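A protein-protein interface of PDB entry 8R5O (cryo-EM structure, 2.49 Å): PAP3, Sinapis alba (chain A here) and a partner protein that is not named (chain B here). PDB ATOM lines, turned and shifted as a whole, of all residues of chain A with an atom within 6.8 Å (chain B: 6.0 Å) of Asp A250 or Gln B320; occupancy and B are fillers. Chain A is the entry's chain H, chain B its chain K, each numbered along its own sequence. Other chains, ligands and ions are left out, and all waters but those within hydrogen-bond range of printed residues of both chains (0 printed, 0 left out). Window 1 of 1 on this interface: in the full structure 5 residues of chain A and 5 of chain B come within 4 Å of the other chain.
NE2 of Gln A249 sits at hydrogen-bond distance from OD2 of Asp A250 (3.1 Å). The backbone carbonyl oxygen (O) of Gln A249 sits at hydrogen-bond distance from the guanidinium group (NH2) of Arg A258, 3.0 Å away.
Of the 11 printed residues of chain A, 4 touch a printed residue of chain B. Printed residues of chain A that touch a printed residue of chain B: Gln A249, Asp A250, Tyr A252 and Phe A363. Hydrophobic or aromatic side chains of chain A that line the printed part of chain B: Tyr A252 and Phe A363. Among the printed residues, 10 pairs touch across the chains. Among the printed residues, no Asp or Glu carboxylate lies within 4 Å of a Lys or Arg side-chain nitrogen of the other chain.
The side-chain hydroxyl of Tyr B317 lies within hydrogen-bond range of the side-chain carboxylate of Asp A250, 2.7 Å away. The backbone carbonyl oxygen (O) of Thr B318 sits at hydrogen-bond distance from the side-chain amide nitrogen (NE2) of Gln A249 (2.7 Å). N of Gln B320 is in hydrogen-bond range of OD2 of Asp A250, at 2.6 Å.
Of chain B, only Tyr B317, Pro B319, Gln B320 and Tyr B321 come within 4 Å of Asp A250. Phe A251 touches none of the printed residues of chain B. Of the printed residues of chain B, Tyr A252 touches Tyr B321. Arg A365 touches none of the printed residues of chain B. Printed residues of chain A within 4 Å of Tyr B317: Gln A249 (3.3 Å) and Asp A250 (2.7 Å). Of the printed residues of chain A, Thr B318 touches Gln A249. Printed residues of chain A within 4 Å of Pro B319: Gln A249 and Asp A250. Gln B320 touches two residues of chain A. Printed residues of chain A within 4 Å of Tyr B321: Asp A250, Tyr A252 and Phe A363. The nearest printed residue of chain A that does not touch Gln B320 is Asp A248 (4.5 Å). The nearest printed residue of chain A that does not touch Pro B319 is Phe A251 (8.7 Å).
Gln A249 touches Tyr B317. Pro B319 touches Gln A249. Gln A249 touches Gln B320 (N to OE1, 3.6 Å). Asp A250 touches Pro B319. Asp A250 touches Tyr B321. CE2 of Tyr B321 touches CB of Tyr A252, at 3.5 Å. OH of Tyr B321 touches CE1 of Phe A363, at 3.7 Å.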
ATOM      1  N   SER A 244      13.391 -25.092  38.819  1.00  0.00           N
ATOM      2  CA  SER A 244      14.108 -25.363  37.577  1.00  0.00           C
ATOM      3  C   SER A 244      13.388 -24.753  36.381  1.00  0.00           C
ATOM      4  O   SER A 244      14.024 -24.160  35.502  1.00  0.00           O
ATOM      5  CB  SER A 244      14.281 -26.871  37.393  1.00  0.00           C
ATOM      6  OG  SER A 244      15.047 -27.159  36.237  1.00  0.00           O
ATOM      7  N   TYR A 247      13.665 -20.771  36.466  1.00  0.00           N
ATOM      8  CA  TYR A 247      14.975 -20.185  36.218  1.00  0.00           C
ATOM      9  C   TYR A 247      15.610 -20.640  34.910  1.00  0.00           C
ATOM     10  O   TYR A 247      16.240 -19.831  34.225  1.00  0.00           O
ATOM     11  CB  TYR A 247      15.919 -20.510  37.379  1.00  0.00           C
ATOM     12  CG  TYR A 247      15.493 -19.902  38.694  1.00  0.00           C
ATOM     13  CD1 TYR A 247      15.052 -18.587  38.761  1.00  0.00           C
ATOM     14  CD2 TYR A 247      15.519 -20.644  39.866  1.00  0.00           C
ATOM     15  CE1 TYR A 247      14.657 -18.027  39.960  1.00  0.00           C
ATOM     16  CE2 TYR A 247      15.125 -20.093  41.068  1.00  0.00           C
ATOM     17  CZ  TYR A 247      14.696 -18.784  41.110  1.00  0.00           C
ATOM     18  OH  TYR A 247      14.305 -18.234  42.309  1.00  0.00           O
ATOM     19  N   ASP A 248      15.464 -21.910  34.546  1.00  0.00           N
ATOM     20  CA  ASP A 248      16.114 -22.473  33.367  1.00  0.00           C
ATOM     21  C   ASP A 248      15.060 -22.717  32.295  1.00  0.00           C
ATOM     22  O   ASP A 248      14.184 -23.573  32.459  1.00  0.00           O
ATOM     23  CB  ASP A 248      16.855 -23.760  33.722  1.00  0.00           C
ATOM     24  CG  ASP A 248      17.893 -23.550  34.808  1.00  0.00           C
ATOM     25  OD1 ASP A 248      18.504 -22.462  34.846  1.00  0.00           O
ATOM     26  OD2 ASP A 248      18.095 -24.470  35.627  1.00  0.00           O
ATOM     27  N   GLN A 249      15.147 -21.962  31.198  1.00  0.00           N
ATOM     28  CA  GLN A 249      14.155 -22.078  30.134  1.00  0.00           C
ATOM     29  C   GLN A 249      14.275 -23.410  29.403  1.00  0.00           C
ATOM     30  O   GLN A 249      13.277 -24.110  29.201  1.00  0.00           O
ATOM     31  CB  GLN A 249      14.304 -20.914  29.154  1.00  0.00           C
ATOM     32  CG  GLN A 249      13.447 -21.043  27.910  1.00  0.00           C
ATOM     33  CD  GLN A 249      13.840 -20.057  26.833  1.00  0.00           C
ATOM     34  OE1 GLN A 249      13.754 -18.845  27.023  1.00  0.00           O
ATOM     35  NE2 GLN A 249      14.281 -20.572  25.693  1.00  0.00           N
ATOM     36  N   ASP A 250      15.486 -23.775  28.997  1.00  0.00           N
ATOM     37  CA  ASP A 250      15.725 -24.990  28.235  1.00  0.00           C
ATOM     38  C   ASP A 250      16.636 -25.923  29.014  1.00  0.00           C
ATOM     39  O   ASP A 250      17.474 -25.484  29.806  1.00  0.00           O
ATOM     40  CB  ASP A 250      16.353 -24.685  26.870  1.00  0.00           C
ATOM     41  CG  ASP A 250      15.413 -23.936  25.948  1.00  0.00           C
ATOM     42  OD1 ASP A 250      14.187 -24.155  26.039  1.00  0.00           O
ATOM     43  OD2 ASP A 250      15.901 -23.131  25.129  1.00  0.00           O
ATOM     44  N   PHE A 251      16.463 -27.220  28.784  1.00  0.00           N
ATOM     45  CA  PHE A 251      17.340 -28.196  29.404  1.00  0.00           C
ATOM     46  C   PHE A 251      18.700 -28.209  28.716  1.00  0.00           C
ATOM     47  O   PHE A 251      18.823 -27.955  27.516  1.00  0.00           O
ATOM     48  CB  PHE A 251      16.722 -29.592  29.360  1.00  0.00           C
ATOM     49  CG  PHE A 251      17.592 -30.648  29.972  1.00  0.00           C
ATOM     50  CD1 PHE A 251      17.693 -30.767  31.348  1.00  0.00           C
ATOM     51  CD2 PHE A 251      18.321 -31.511  29.175  1.00  0.00           C
ATOM     52  CE1 PHE A 251      18.498 -31.731  31.915  1.00  0.00           C
ATOM     53  CE2 PHE A 251      19.128 -32.477  29.736  1.00  0.00           C
ATOM     54  CZ  PHE A 251      19.216 -32.589  31.108  1.00  0.00           C
ATOM     55  N   TYR A 252      19.729 -28.508  29.502  1.00  0.00           N
ATOM     56  CA  TYR A 252      21.099 -28.610  29.027  1.00  0.00           C
ATOM     57  C   TYR A 252      21.848 -29.494  30.006  1.00  0.00           C
ATOM     58  O   TYR A 252      21.499 -29.516  31.191  1.00  0.00           O
ATOM     59  CB  TYR A 252      21.753 -27.223  28.934  1.00  0.00           C
ATOM     60  CG  TYR A 252      23.048 -27.192  28.162  1.00  0.00           C
ATOM     61  CD1 TYR A 252      23.048 -27.135  26.776  1.00  0.00           C
ATOM     62  CD2 TYR A 252      24.271 -27.219  28.818  1.00  0.00           C
ATOM     63  CE1 TYR A 252      24.227 -27.107  26.066  1.00  0.00           C
ATOM     64  CE2 TYR A 252      25.454 -27.192  28.116  1.00  0.00           C
ATOM     65  CZ  TYR A 252      25.427 -27.135  26.739  1.00  0.00           C
ATOM     66  OH  TYR A 252      26.604 -27.108  26.034  1.00  0.00           O
ATOM     67  N   ARG A 255      21.929 -29.165  33.941  1.00  0.00           N
ATOM     68  CA  ARG A 255      20.683 -28.676  34.507  1.00  0.00           C
ATOM     69  C   ARG A 255      19.917 -29.818  35.168  1.00  0.00           C
ATOM     70  O   ARG A 255      20.264 -30.995  35.043  1.00  0.00           O
ATOM     71  CB  ARG A 255      19.822 -28.010  33.433  1.00  0.00           C
ATOM     72  CG  ARG A 255      20.424 -26.753  32.813  1.00  0.00           C
ATOM     73  CD  ARG A 255      20.548 -25.628  33.827  1.00  0.00           C
ATOM     74  NE  ARG A 255      21.779 -25.712  34.601  1.00  0.00           N
ATOM     75  CZ  ARG A 255      21.972 -25.122  35.772  1.00  0.00           C
ATOM     76  NH1 ARG A 255      21.025 -24.399  36.344  1.00  0.00           N
ATOM     77  NH2 ARG A 255      23.142 -25.266  36.384  1.00  0.00           N
ATOM     78  N   ARG A 258      14.009 -32.920  34.394  1.00  0.00           N
ATOM     79  CA  ARG A 258      12.644 -32.573  34.758  1.00  0.00           C
ATOM     80  C   ARG A 258      11.683 -33.153  33.729  1.00  0.00           C
ATOM     81  O   ARG A 258      12.092 -33.767  32.739  1.00  0.00           O
ATOM     82  CB  ARG A 258      12.485 -31.053  34.863  1.00  0.00           C
ATOM     83  CG  ARG A 258      12.783 -30.328  33.564  1.00  0.00           C
ATOM     84  CD  ARG A 258      13.074 -28.861  33.792  1.00  0.00           C
ATOM     85  NE  ARG A 258      13.265 -28.152  32.533  1.00  0.00           N
ATOM     86  CZ  ARG A 258      13.605 -26.875  32.435  1.00  0.00           C
ATOM     87  NH1 ARG A 258      13.823 -26.134  33.508  1.00  0.00           N
ATOM     88  NH2 ARG A 258      13.727 -26.328  31.230  1.00  0.00           N
ATOM     89  N   PHE A 363      26.227 -18.488  35.325  1.00  0.00           N
ATOM     90  CA  PHE A 363      25.109 -17.798  34.695  1.00  0.00           C
ATOM     91  C   PHE A 363      25.136 -16.320  35.057  1.00  0.00           C
ATOM     92  O   PHE A 363      25.486 -15.949  36.179  1.00  0.00           O
ATOM     93  CB  PHE A 363      23.770 -18.391  35.138  1.00  0.00           C
ATOM     94  CG  PHE A 363      23.488 -19.758  34.592  1.00  0.00           C
ATOM     95  CD1 PHE A 363      22.997 -19.918  33.309  1.00  0.00           C
ATOM     96  CD2 PHE A 363      23.682 -20.883  35.375  1.00  0.00           C
ATOM     97  CE1 PHE A 363      22.726 -21.173  32.809  1.00  0.00           C
ATOM     98  CE2 PHE A 363      23.410 -22.140  34.880  1.00  0.00           C
ATOM     99  CZ  PHE A 363      22.932 -22.285  33.595  1.00  0.00           C
ATOM    100  N   ARG A 365      22.273 -13.793  35.353  1.00  0.00           N
ATOM    101  CA  ARG A 365      20.825 -13.911  35.394  1.00  0.00           C
ATOM    102  C   ARG A 365      20.165 -12.541  35.540  1.00  0.00           C
ATOM    103  O   ARG A 365      20.823 -11.498  35.560  1.00  0.00           O
ATOM    104  CB  ARG A 365      20.407 -14.852  36.525  1.00  0.00           C
ATOM    105  CG  ARG A 365      21.233 -16.126  36.593  1.00  0.00           C
ATOM    106  CD  ARG A 365      20.551 -17.191  37.425  1.00  0.00           C
ATOM    107  NE  ARG A 365      19.509 -17.880  36.676  1.00  0.00           N
ATOM    108  CZ  ARG A 365      19.590 -19.136  36.259  1.00  0.00           C
ATOM    109  NH1 ARG A 365      20.638 -19.890  36.538  1.00  0.00           N
ATOM    110  NH2 ARG A 365      18.589 -19.649  35.551  1.00  0.00           N
ATOM    111  N   TYR B 317       9.267 -17.094  21.492  1.00  0.00           N
ATOM    112  CA  TYR B 317      10.168 -18.083  22.069  1.00  0.00           C
ATOM    113  C   TYR B 317      11.459 -18.159  21.265  1.00  0.00           C
ATOM    114  O   TYR B 317      11.432 -18.199  20.031  1.00  0.00           O
ATOM    115  CB  TYR B 317       9.499 -19.454  22.119  1.00  0.00           C
ATOM    116  CG  TYR B 317      10.431 -20.566  22.542  1.00  0.00           C
ATOM    117  CD1 TYR B 317      10.731 -20.774  23.880  1.00  0.00           C
ATOM    118  CD2 TYR B 317      11.010 -21.408  21.603  1.00  0.00           C
ATOM    119  CE1 TYR B 317      11.582 -21.786  24.272  1.00  0.00           C
ATOM    120  CE2 TYR B 317      11.864 -22.426  21.986  1.00  0.00           C
ATOM    121  CZ  TYR B 317      12.145 -22.609  23.322  1.00  0.00           C
ATOM    122  OH  TYR B 317      12.993 -23.620  23.712  1.00  0.00           O
ATOM    123  N   THR B 318      12.589 -18.181  21.969  1.00  0.00           N
ATOM    124  CA  THR B 318      13.897 -18.337  21.356  1.00  0.00           C
ATOM    125  C   THR B 318      14.672 -19.392  22.136  1.00  0.00           C
ATOM    126  O   THR B 318      14.786 -19.287  23.369  1.00  0.00           O
ATOM    127  CB  THR B 318      14.669 -17.011  21.339  1.00  0.00           C
ATOM    128  OG1 THR B 318      13.902 -16.020  20.647  1.00  0.00           O
ATOM    129  CG2 THR B 318      16.008 -17.184  20.643  1.00  0.00           C
ATOM    130  N   PRO B 319      15.202 -20.420  21.474  1.00  0.00           N
ATOM    131  CA  PRO B 319      15.983 -21.434  22.194  1.00  0.00           C
ATOM    132  C   PRO B 319      17.200 -20.820  22.871  1.00  0.00           C
ATOM    133  O   PRO B 319      17.831 -19.901  22.348  1.00  0.00           O
ATOM    134  CB  PRO B 319      16.378 -22.428  21.095  1.00  0.00           C
ATOM    135  CG  PRO B 319      16.189 -21.691  19.812  1.00  0.00           C
ATOM    136  CD  PRO B 319      15.073 -20.732  20.042  1.00  0.00           C
ATOM    137  N   GLN B 320      17.519 -21.341  24.056  1.00  0.00           N
ATOM    138  CA  GLN B 320      18.521 -20.708  24.906  1.00  0.00           C
ATOM    139  C   GLN B 320      19.944 -20.990  24.435  1.00  0.00           C
ATOM    140  O   GLN B 320      20.806 -20.108  24.507  1.00  0.00           O
ATOM    141  CB  GLN B 320      18.336 -21.167  26.352  1.00  0.00           C
ATOM    142  CG  GLN B 320      19.229 -20.459  27.347  1.00  0.00           C
ATOM    143  CD  GLN B 320      18.869 -20.782  28.781  1.00  0.00           C
ATOM    144  OE1 GLN B 320      17.966 -21.576  29.041  1.00  0.00           O
ATOM    145  NE2 GLN B 320      19.572 -20.164  29.721  1.00  0.00           N
ATOM    146  N   TYR B 321      20.214 -22.201  23.953  1.00  0.00           N
ATOM    147  CA  TYR B 321      21.574 -22.616  23.634  1.00  0.00           C
ATOM    148  C   TYR B 321      21.811 -22.814  22.145  1.00  0.00           C
ATOM    149  O   TYR B 321      22.777 -22.277  21.598  1.00  0.00           O
ATOM    150  CB  TYR B 321      21.915 -23.904  24.397  1.00  0.00           C
ATOM    151  CG  TYR B 321      21.809 -23.754  25.896  1.00  0.00           C
ATOM    152  CD1 TYR B 321      22.832 -23.172  26.629  1.00  0.00           C
ATOM    153  CD2 TYR B 321      20.681 -24.190  26.578  1.00  0.00           C
ATOM    154  CE1 TYR B 321      22.737 -23.029  27.998  1.00  0.00           C
ATOM    155  CE2 TYR B 321      20.577 -24.051  27.945  1.00  0.00           C
ATOM    156  CZ  TYR B 321      21.609 -23.472  28.651  1.00  0.00           C
ATOM    157  OH  TYR B 321      21.512 -23.332  30.015  1.00  0.00           O
ATOM    158  N   PHE B 322      20.956 -23.577  21.469  1.00  0.00           N
ATOM    159  CA  PHE B 322      21.114 -23.804  20.042  1.00  0.00           C
ATOM    160  C   PHE B 322      19.749 -24.053  19.421  1.00  0.00           C
ATOM    161  O   PHE B 322      18.798 -24.444  20.100  1.00  0.00           O
ATOM    162  CB  PHE B 322      22.062 -24.977  19.759  1.00  0.00           C
ATOM    163  CG  PHE B 322      21.806 -26.184  20.613  1.00  0.00           C
ATOM    164  CD1 PHE B 322      20.822 -27.095  20.273  1.00  0.00           C
ATOM    165  CD2 PHE B 322      22.555 -26.409  21.755  1.00  0.00           C
ATOM    166  CE1 PHE B 322      20.587 -28.203  21.058  1.00  0.00           C
ATOM    167  CE2 PHE B 322      22.323 -27.517  22.544  1.00  0.00           C
ATOM    168  CZ  PHE B 322      21.338 -28.415  22.195  1.00  0.00           C
